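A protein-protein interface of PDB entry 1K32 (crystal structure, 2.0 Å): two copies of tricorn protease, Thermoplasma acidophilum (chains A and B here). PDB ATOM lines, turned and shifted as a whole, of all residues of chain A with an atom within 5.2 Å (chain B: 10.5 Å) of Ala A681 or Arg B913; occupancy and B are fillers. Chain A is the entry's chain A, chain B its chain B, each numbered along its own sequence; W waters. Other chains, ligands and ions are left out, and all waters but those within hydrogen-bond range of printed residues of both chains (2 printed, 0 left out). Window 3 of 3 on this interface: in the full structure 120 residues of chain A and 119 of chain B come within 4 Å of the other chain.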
ATOM      1  N   ARG A 672      -6.393 -17.483  21.077  1.00  0.00           N
ATOM      2  CA  ARG A 672      -6.779 -18.622  21.890  1.00  0.00           C
ATOM      3  C   ARG A 672      -7.970 -18.342  22.805  1.00  0.00           C
ATOM      4  O   ARG A 672      -8.965 -19.063  22.780  1.00  0.00           O
ATOM      5  CB  ARG A 672      -5.612 -19.078  22.752  1.00  0.00           C
ATOM      6  CG  ARG A 672      -5.937 -20.312  23.570  1.00  0.00           C
ATOM      7  CD  ARG A 672      -4.925 -20.494  24.669  1.00  0.00           C
ATOM      8  NE  ARG A 672      -4.942 -19.361  25.589  1.00  0.00           N
ATOM      9  CZ  ARG A 672      -4.143 -19.254  26.643  1.00  0.00           C
ATOM     10  NH1 ARG A 672      -4.221 -18.193  27.431  1.00  0.00           N
ATOM     11  NH2 ARG A 672      -3.263 -20.216  26.909  1.00  0.00           N
ATOM     12  N   ASP A 673      -7.843 -17.303  23.623  1.00  0.00           N
ATOM     13  CA  ASP A 673      -8.884 -16.918  24.575  1.00  0.00           C
ATOM     14  C   ASP A 673     -10.249 -16.636  23.968  1.00  0.00           C
ATOM     15  O   ASP A 673     -11.273 -16.940  24.581  1.00  0.00           O
ATOM     16  CB  ASP A 673      -8.467 -15.662  25.347  1.00  0.00           C
ATOM     17  CG  ASP A 673      -7.336 -15.915  26.306  1.00  0.00           C
ATOM     18  OD1 ASP A 673      -6.863 -14.936  26.922  1.00  0.00           O
ATOM     19  OD2 ASP A 673      -6.926 -17.084  26.447  1.00  0.00           O
ATOM     20  N   ASN A 674     -10.273 -16.044  22.779  1.00  0.00           N
ATOM     21  CA  ASN A 674     -11.544 -15.680  22.172  1.00  0.00           C
ATOM     22  C   ASN A 674     -12.105 -16.591  21.105  1.00  0.00           C
ATOM     23  O   ASN A 674     -13.240 -16.390  20.658  1.00  0.00           O
ATOM     24  CB  ASN A 674     -11.470 -14.246  21.638  1.00  0.00           C
ATOM     25  CG  ASN A 674     -11.203 -13.237  22.742  1.00  0.00           C
ATOM     26  OD1 ASN A 674     -11.628 -13.427  23.883  1.00  0.00           O
ATOM     27  ND2 ASN A 674     -10.501 -12.164  22.410  1.00  0.00           N
ATOM     28  N   TYR A 675     -11.332 -17.590  20.691  1.00  0.00           N
ATOM     29  CA  TYR A 675     -11.830 -18.500  19.681  1.00  0.00           C
ATOM     30  C   TYR A 675     -13.179 -19.003  20.190  1.00  0.00           C
ATOM     31  O   TYR A 675     -13.349 -19.216  21.399  1.00  0.00           O
ATOM     32  CB  TYR A 675     -10.857 -19.661  19.472  1.00  0.00           C
ATOM     33  CG  TYR A 675     -11.236 -20.487  18.276  1.00  0.00           C
ATOM     34  CD1 TYR A 675     -11.360 -19.887  17.014  1.00  0.00           C
ATOM     35  CD2 TYR A 675     -11.537 -21.843  18.402  1.00  0.00           C
ATOM     36  CE1 TYR A 675     -11.782 -20.611  15.911  1.00  0.00           C
ATOM     37  CE2 TYR A 675     -11.962 -22.590  17.291  1.00  0.00           C
ATOM     38  CZ  TYR A 675     -12.086 -21.959  16.054  1.00  0.00           C
ATOM     39  OH  TYR A 675     -12.558 -22.647  14.969  1.00  0.00           O
ATOM     40  N   TRP A 676     -14.142 -19.191  19.291  1.00  0.00           N
ATOM     41  CA  TRP A 676     -15.474 -19.616  19.721  1.00  0.00           C
ATOM     42  C   TRP A 676     -15.567 -20.960  20.443  1.00  0.00           C
ATOM     43  O   TRP A 676     -16.385 -21.110  21.345  1.00  0.00           O
ATOM     44  CB  TRP A 676     -16.460 -19.634  18.544  1.00  0.00           C
ATOM     45  CG  TRP A 676     -16.330 -20.829  17.644  1.00  0.00           C
ATOM     46  CD1 TRP A 676     -15.433 -20.997  16.632  1.00  0.00           C
ATOM     47  CD2 TRP A 676     -17.160 -22.000  17.644  1.00  0.00           C
ATOM     48  NE1 TRP A 676     -15.658 -22.190  15.994  1.00  0.00           N
ATOM     49  CE2 TRP A 676     -16.711 -22.827  16.593  1.00  0.00           C
ATOM     50  CE3 TRP A 676     -18.242 -22.428  18.430  1.00  0.00           C
ATOM     51  CZ2 TRP A 676     -17.307 -24.063  16.300  1.00  0.00           C
ATOM     52  CZ3 TRP A 676     -18.840 -23.664  18.137  1.00  0.00           C
ATOM     53  CH2 TRP A 676     -18.368 -24.461  17.082  1.00  0.00           C
ATOM     54  N   ASN A 677     -14.746 -21.923  20.034  1.00  0.00           N
ATOM     55  CA  ASN A 677     -14.754 -23.267  20.611  1.00  0.00           C
ATOM     56  C   ASN A 677     -13.546 -23.469  21.530  1.00  0.00           C
ATOM     57  O   ASN A 677     -12.434 -23.740  21.075  1.00  0.00           O
ATOM     58  CB  ASN A 677     -14.756 -24.289  19.467  1.00  0.00           C
ATOM     59  CG  ASN A 677     -14.857 -25.725  19.946  1.00  0.00           C
ATOM     60  OD1 ASN A 677     -15.034 -26.639  19.143  1.00  0.00           O
ATOM     61  ND2 ASN A 677     -14.741 -25.934  21.244  1.00  0.00           N
ATOM     62  N   GLU A 678     -13.773 -23.331  22.832  1.00  0.00           N
ATOM     63  CA  GLU A 678     -12.700 -23.474  23.808  1.00  0.00           C
ATOM     64  C   GLU A 678     -11.983 -24.825  23.729  1.00  0.00           C
ATOM     65  O   GLU A 678     -10.762 -24.886  23.834  1.00  0.00           O
ATOM     66  CB  GLU A 678     -13.241 -23.246  25.227  1.00  0.00           C
ATOM     67  CG  GLU A 678     -12.169 -23.291  26.307  1.00  0.00           C
ATOM     68  CD  GLU A 678     -12.732 -23.134  27.710  1.00  0.00           C
ATOM     69  OE1 GLU A 678     -11.936 -23.136  28.673  1.00  0.00           O
ATOM     70  OE2 GLU A 678     -13.969 -23.009  27.852  1.00  0.00           O
ATOM     71  N   ALA A 679     -12.730 -25.905  23.530  1.00  0.00           N
ATOM     72  CA  ALA A 679     -12.116 -27.231  23.442  1.00  0.00           C
ATOM     73  C   ALA A 679     -10.994 -27.235  22.402  1.00  0.00           C
ATOM     74  O   ALA A 679      -9.855 -27.608  22.680  1.00  0.00           O
ATOM     75  CB  ALA A 679     -13.170 -28.272  23.069  1.00  0.00           C
ATOM     76  N   VAL A 680     -11.336 -26.799  21.201  1.00  0.00           N
ATOM     77  CA  VAL A 680     -10.399 -26.743  20.097  1.00  0.00           C
ATOM     78  C   VAL A 680      -9.271 -25.728  20.292  1.00  0.00           C
ATOM     79  O   VAL A 680      -8.141 -25.964  19.862  1.00  0.00           O
ATOM     80  CB  VAL A 680     -11.167 -26.421  18.800  1.00  0.00           C
ATOM     81  CG1 VAL A 680     -10.219 -26.286  17.631  1.00  0.00           C
ATOM     82  CG2 VAL A 680     -12.183 -27.517  18.540  1.00  0.00           C
ATOM     83  N   ALA A 681      -9.576 -24.609  20.946  1.00  0.00           N
ATOM     84  CA  ALA A 681      -8.595 -23.543  21.169  1.00  0.00           C
ATOM     85  C   ALA A 681      -7.325 -23.953  21.926  1.00  0.00           C
ATOM     86  O   ALA A 681      -6.224 -23.494  21.609  1.00  0.00           O
ATOM     87  CB  ALA A 681      -9.265 -22.375  21.882  1.00  0.00           C
ATOM     88  N   LYS A 682      -7.473 -24.805  22.935  1.00  0.00           N
ATOM     89  CA  LYS A 682      -6.327 -25.257  23.715  1.00  0.00           C
ATOM     90  C   LYS A 682      -5.336 -26.033  22.847  1.00  0.00           C
ATOM     91  O   LYS A 682      -4.135 -25.753  22.859  1.00  0.00           O
ATOM     92  N   GLU A 683      -5.842 -27.001  22.088  1.00  0.00           N
ATOM     93  CA  GLU A 683      -5.001 -27.832  21.226  1.00  0.00           C
ATOM     94  C   GLU A 683      -4.309 -27.061  20.093  1.00  0.00           C
ATOM     95  O   GLU A 683      -3.127 -27.268  19.822  1.00  0.00           O
ATOM     96  CB  GLU A 683      -5.848 -28.975  20.645  1.00  0.00           C
ATOM     97  CG  GLU A 683      -5.086 -30.040  19.840  1.00  0.00           C
ATOM     98  CD  GLU A 683      -4.782 -29.618  18.400  1.00  0.00           C
ATOM     99  OE1 GLU A 683      -5.632 -28.946  17.771  1.00  0.00           O
ATOM    100  OE2 GLU A 683      -3.696 -29.977  17.890  1.00  0.00           O
ATOM    101  N   ILE A 684      -5.047 -26.175  19.433  1.00  0.00           N
ATOM    102  CA  ILE A 684      -4.490 -25.411  18.329  1.00  0.00           C
ATOM    103  C   ILE A 684      -3.413 -24.434  18.790  1.00  0.00           C
ATOM    104  O   ILE A 684      -2.312 -24.416  18.238  1.00  0.00           O
ATOM    105  CB  ILE A 684      -5.599 -24.629  17.570  1.00  0.00           C
ATOM    106  CG1 ILE A 684      -6.531 -25.622  16.865  1.00  0.00           C
ATOM    107  CG2 ILE A 684      -4.970 -23.667  16.555  1.00  0.00           C
ATOM    108  CD1 ILE A 684      -7.758 -24.979  16.231  1.00  0.00           C
ATOM    109  N   SER A 685      -3.723 -23.636  19.807  1.00  0.00           N
ATOM    110  CA  SER A 685      -2.764 -22.657  20.303  1.00  0.00           C
ATOM    111  C   SER A 685      -1.434 -23.285  20.746  1.00  0.00           C
ATOM    112  O   SER A 685      -0.367 -22.777  20.410  1.00  0.00           O
ATOM    113  CB  SER A 685      -3.366 -21.844  21.457  1.00  0.00           C
ATOM    114  OG  SER A 685      -3.596 -22.643  22.598  1.00  0.00           O
ATOM    115  N   GLU A 686      -1.498 -24.388  21.486  1.00  0.00           N
ATOM    116  CA  GLU A 686      -0.286 -25.043  21.967  1.00  0.00           C
ATOM    117  C   GLU A 686       0.525 -25.663  20.842  1.00  0.00           C
ATOM    118  O   GLU A 686       1.743 -25.776  20.928  1.00  0.00           O
ATOM    119  CB  GLU A 686      -0.647 -26.123  22.983  1.00  0.00           C
ATOM    120  CG  GLU A 686      -1.321 -25.577  24.211  1.00  0.00           C
ATOM    121  CD  GLU A 686      -1.487 -26.627  25.287  1.00  0.00           C
ATOM    122  OE1 GLU A 686      -2.224 -27.615  25.052  1.00  0.00           O
ATOM    123  OE2 GLU A 686      -0.872 -26.462  26.364  1.00  0.00           O
ATOM    124  N   TYR A 716      -6.157 -21.338  12.792  1.00  0.00           N
ATOM    125  CA  TYR A 716      -7.444 -21.623  13.392  1.00  0.00           C
ATOM    126  C   TYR A 716      -8.420 -22.119  12.338  1.00  0.00           C
ATOM    127  O   TYR A 716      -9.514 -22.585  12.664  1.00  0.00           O
ATOM    128  CB  TYR A 716      -7.979 -20.389  14.135  1.00  0.00           C
ATOM    129  CG  TYR A 716      -7.400 -20.284  15.532  1.00  0.00           C
ATOM    130  CD1 TYR A 716      -6.164 -19.674  15.767  1.00  0.00           C
ATOM    131  CD2 TYR A 716      -8.039 -20.907  16.606  1.00  0.00           C
ATOM    132  CE1 TYR A 716      -5.573 -19.699  17.039  1.00  0.00           C
ATOM    133  CE2 TYR A 716      -7.467 -20.944  17.864  1.00  0.00           C
ATOM    134  CZ  TYR A 716      -6.236 -20.349  18.080  1.00  0.00           C
ATOM    135  OH  TYR A 716      -5.671 -20.466  19.331  1.00  0.00           O
ATOM    136  N   GLU A 984     -15.146 -15.466  17.342  1.00  0.00           N
ATOM    137  CA  GLU A 984     -15.711 -15.723  18.649  1.00  0.00           C
ATOM    138  C   GLU A 984     -17.162 -16.177  18.730  1.00  0.00           C
ATOM    139  O   GLU A 984     -17.575 -16.747  19.743  1.00  0.00           O
ATOM    140  CB  GLU A 984     -15.518 -14.450  19.476  1.00  0.00           C
ATOM    141  CG  GLU A 984     -15.715 -14.614  20.960  1.00  0.00           C
ATOM    142  CD  GLU A 984     -15.385 -13.350  21.722  1.00  0.00           C
ATOM    143  OE1 GLU A 984     -14.467 -12.624  21.308  1.00  0.00           O
ATOM    144  OE2 GLU A 984     -16.042 -13.088  22.744  1.00  0.00           O
ATOM    145  N   ASP B 910     -26.348 -17.840  17.600  1.00  0.00           N
ATOM    146  CA  ASP B 910     -24.914 -17.622  17.611  1.00  0.00           C
ATOM    147  C   ASP B 910     -24.464 -18.377  18.852  1.00  0.00           C
ATOM    148  O   ASP B 910     -25.211 -18.475  19.821  1.00  0.00           O
ATOM    149  CB  ASP B 910     -24.579 -16.140  17.755  1.00  0.00           C
ATOM    150  CG  ASP B 910     -24.373 -15.464  16.414  1.00  0.00           C
ATOM    151  OD1 ASP B 910     -25.016 -14.420  16.171  1.00  0.00           O
ATOM    152  OD2 ASP B 910     -23.564 -15.985  15.609  1.00  0.00           O
ATOM    153  N   ASN B 911     -23.260 -18.928  18.803  1.00  0.00           N
ATOM    154  CA  ASN B 911     -22.697 -19.668  19.920  1.00  0.00           C
ATOM    155  C   ASN B 911     -21.393 -18.968  20.273  1.00  0.00           C
ATOM    156  O   ASN B 911     -20.386 -19.099  19.573  1.00  0.00           O
ATOM    157  CB  ASN B 911     -22.453 -21.117  19.513  1.00  0.00           C
ATOM    158  CG  ASN B 911     -23.722 -21.805  19.037  1.00  0.00           C
ATOM    159  OD1 ASN B 911     -24.290 -21.448  17.995  1.00  0.00           O
ATOM    160  ND2 ASN B 911     -24.185 -22.782  19.807  1.00  0.00           N
ATOM    161  N   PRO B 912     -21.397 -18.208  21.374  1.00  0.00           N
ATOM    162  CA  PRO B 912     -20.215 -17.473  21.811  1.00  0.00           C
ATOM    163  C   PRO B 912     -19.244 -18.265  22.666  1.00  0.00           C
ATOM    164  O   PRO B 912     -19.605 -19.279  23.264  1.00  0.00           O
ATOM    165  CB  PRO B 912     -20.822 -16.303  22.567  1.00  0.00           C
ATOM    166  CG  PRO B 912     -21.970 -16.967  23.286  1.00  0.00           C
ATOM    167  CD  PRO B 912     -22.553 -17.920  22.247  1.00  0.00           C
ATOM    168  N   ARG B 913     -17.998 -17.800  22.706  1.00  0.00           N
ATOM    169  CA  ARG B 913     -16.984 -18.447  23.521  1.00  0.00           C
ATOM    170  C   ARG B 913     -17.426 -18.276  24.971  1.00  0.00           C
ATOM    171  O   ARG B 913     -17.292 -19.185  25.783  1.00  0.00           O
ATOM    172  CB  ARG B 913     -15.627 -17.783  23.306  1.00  0.00           C
ATOM    173  CG  ARG B 913     -14.543 -18.211  24.293  1.00  0.00           C
ATOM    174  CD  ARG B 913     -14.372 -19.731  24.369  1.00  0.00           C
ATOM    175  NE  ARG B 913     -13.219 -20.043  25.207  1.00  0.00           N
ATOM    176  CZ  ARG B 913     -11.953 -20.004  24.802  1.00  0.00           C
ATOM    177  NH1 ARG B 913     -10.980 -20.284  25.661  1.00  0.00           N
ATOM    178  NH2 ARG B 913     -11.654 -19.717  23.537  1.00  0.00           N
ATOM    179  N   ARG B 914     -17.958 -17.099  25.279  1.00  0.00           N
ATOM    180  CA  ARG B 914     -18.450 -16.803  26.614  1.00  0.00           C
ATOM    181  C   ARG B 914     -19.828 -16.146  26.526  1.00  0.00           C
ATOM    182  O   ARG B 914     -20.126 -15.417  25.576  1.00  0.00           O
ATOM    183  CB  ARG B 914     -17.462 -15.903  27.364  1.00  0.00           C
ATOM    184  CG  ARG B 914     -17.066 -14.627  26.641  1.00  0.00           C
ATOM    185  CD  ARG B 914     -15.934 -13.913  27.381  1.00  0.00           C
ATOM    186  NE  ARG B 914     -14.744 -14.751  27.475  1.00  0.00           N
ATOM    187  CZ  ARG B 914     -13.838 -14.887  26.506  1.00  0.00           C
ATOM    188  NH1 ARG B 914     -12.789 -15.680  26.679  1.00  0.00           N
ATOM    189  NH2 ARG B 914     -13.966 -14.216  25.366  1.00  0.00           N
ATOM    190  N   GLY B 915     -20.666 -16.421  27.517  1.00  0.00           N
ATOM    191  CA  GLY B 915     -22.008 -15.874  27.523  1.00  0.00           C
ATOM    192  C   GLY B 915     -22.988 -16.921  27.040  1.00  0.00           C
ATOM    193  O   GLY B 915     -22.639 -18.088  26.939  1.00  0.00           O
ATOM    194  N   THR B 916     -24.205 -16.506  26.712  1.00  0.00           N
ATOM    195  CA  THR B 916     -25.234 -17.443  26.275  1.00  0.00           C
ATOM    196  C   THR B 916     -25.591 -17.328  24.794  1.00  0.00           C
ATOM    197  O   THR B 916     -25.160 -16.397  24.119  1.00  0.00           O
ATOM    198  CB  THR B 916     -26.502 -17.249  27.115  1.00  0.00           C
ATOM    199  OG1 THR B 916     -27.024 -15.936  26.896  1.00  0.00           O
ATOM    200  CG2 THR B 916     -26.172 -17.391  28.602  1.00  0.00           C
ATOM    201  N   LEU B 917     -26.391 -18.276  24.303  1.00  0.00           N
ATOM    202  CA  LEU B 917     -26.815 -18.284  22.905  1.00  0.00           C
ATOM    203  C   LEU B 917     -27.590 -17.019  22.586  1.00  0.00           C
ATOM    204  O   LEU B 917     -28.318 -16.511  23.428  1.00  0.00           O
ATOM    205  CB  LEU B 917     -27.723 -19.483  22.608  1.00  0.00           C
ATOM    206  CG  LEU B 917     -27.182 -20.903  22.778  1.00  0.00           C
ATOM    207  CD1 LEU B 917     -28.278 -21.894  22.425  1.00  0.00           C
ATOM    208  CD2 LEU B 917     -25.971 -21.112  21.883  1.00  0.00           C
ATOM    209  N   SER B 918     -27.421 -16.513  21.371  1.00  0.00           N
ATOM    210  CA  SER B 918     -28.132 -15.318  20.911  1.00  0.00           C
ATOM    211  C   SER B 918     -29.001 -15.810  19.771  1.00  0.00           C
ATOM    212  O   SER B 918     -28.473 -16.248  18.748  1.00  0.00           O
ATOM    213  CB  SER B 918     -27.162 -14.269  20.371  1.00  0.00           C
ATOM    214  OG  SER B 918     -26.215 -13.910  21.343  1.00  0.00           O
HETATM  215  O   HOH W   1     -17.613 -14.735  23.633  1.00  0.00           O
HETATM  216  O   HOH W   2     -11.531 -12.083  26.403  1.00  0.00           O
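O of Arg A672 is in hydrogen-bond range of NH2 of Arg B913 (2.9 Å). O of Asp A673 sits at hydrogen-bond distance from NH2 of Arg B913, at 3.0 Å. O of Asp A673 lies within hydrogen-bond range of NH1 of Arg B914, 2.9 Å away. The guanidinium group (NH2) of Arg B914 sits at hydrogen-bond distance from the side-chain amide oxygen (OD1) of Asn A674, at 2.9 Å. The backbone carbonyl oxygen of Tyr A675 is in hydrogen-bond range of the guanidinium group of Arg B913, 2.8 Å away. The backbone carbonyl oxygen of Glu A984 sits at hydrogen-bond distance from the backbone NH of Arg B913, 3.2 Å away. The guanidinium group (NH2) of Arg B914 lies within salt-bridge range of the side-chain carboxylate (OE2) of Glu A984, at 3.5 Å.
Ala A681 touches just one residue of chain B: Arg B913. Arg B913 touches just these residues of chain A: Arg A672, Asp A673, Asn A674, Tyr A675, Trp A676, Glu A678, Ala A681 and Glu A984. Glu A678 touches just one residue of chain B: Arg B913 (3.2 Å). Ala A679 touches none of the printed residues of chain B. No residue of chain B comes within 4 Å of Val A680. Lys A682 touches none of the printed residues of chain B. No residue of chain B comes within 4 Å of Ile A684. Printed residues of chain A within 4 Å of Pro B912: Glu A984 (3.4 Å). Of the printed residues of chain B, Tyr A675 touches Arg B913. Printed residues of chain B within 4 Å of Asn A674: Arg B913 (3.8 Å) and Arg B914 (2.9 Å). Of the printed residues of chain B, Arg A672 touches Arg B913. Of the printed residues of chain A, Asn B911 touches Glu A984 (3.7 Å). Gly B915 touches none of the printed residues of chain A. The nearest residue of chain B that does not touch Ala A681 is Arg B914 (9.0 Å). The nearest residue of chain A that does not touch Arg B913 is Asn A677 (4.7 Å).
Water W1 lies within hydrogen-bond range of OE2 of Glu A984, N of Arg B914 and N of Arg B913. Water W2 lies within hydrogen-bond range of OD1 of Asn A674 (2.9 Å) and NH2 of Arg B914 (3.4 Å).
No position is printed for both chains. Of the 13 pairs that touch across the chains among the printed residues, none has its exchanged pair printed and touching as well.
Among the printed residues, pairs that only touch across the chains: Glu A678 with Arg B913 (3.2 Å), Glu A984 with Pro B912 (3.4 Å), Trp A676 with Arg B913 (3.5 Å), Glu A984 with Asn B911 (3.7 Å), Asn A674 with Arg B913 (3.8 Å) and Ala A681 with Arg B913 (3.9 Å).
The side-chain carboxylate (OD2) of Asp A673 lies within salt-bridge range of the guanidinium group (NH1) of Arg A672. The side-chain hydroxyl of Tyr A675 lies within hydrogen-bond range of the indole nitrogen of Trp A676 (3.3 Å). The side-chain hydroxyl (OG) of Ser A685 lies within hydrogen-bond range of the backbone carbonyl oxygen (O) of Ala A681 (2.9 Å).
Of the 17 printed residues of chain A, 8 touch a printed residue of chain B. Along chain B the printed residues that touch a printed residue of chain A span positions 911 to 914. Among the printed residues, 13 pairs touch across the chains. Among the printed residues, Asp or Glu carboxylates within 4 Å of a Lys or Arg side-chain nitrogen of the other chain: Glu A984 with Arg B914.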
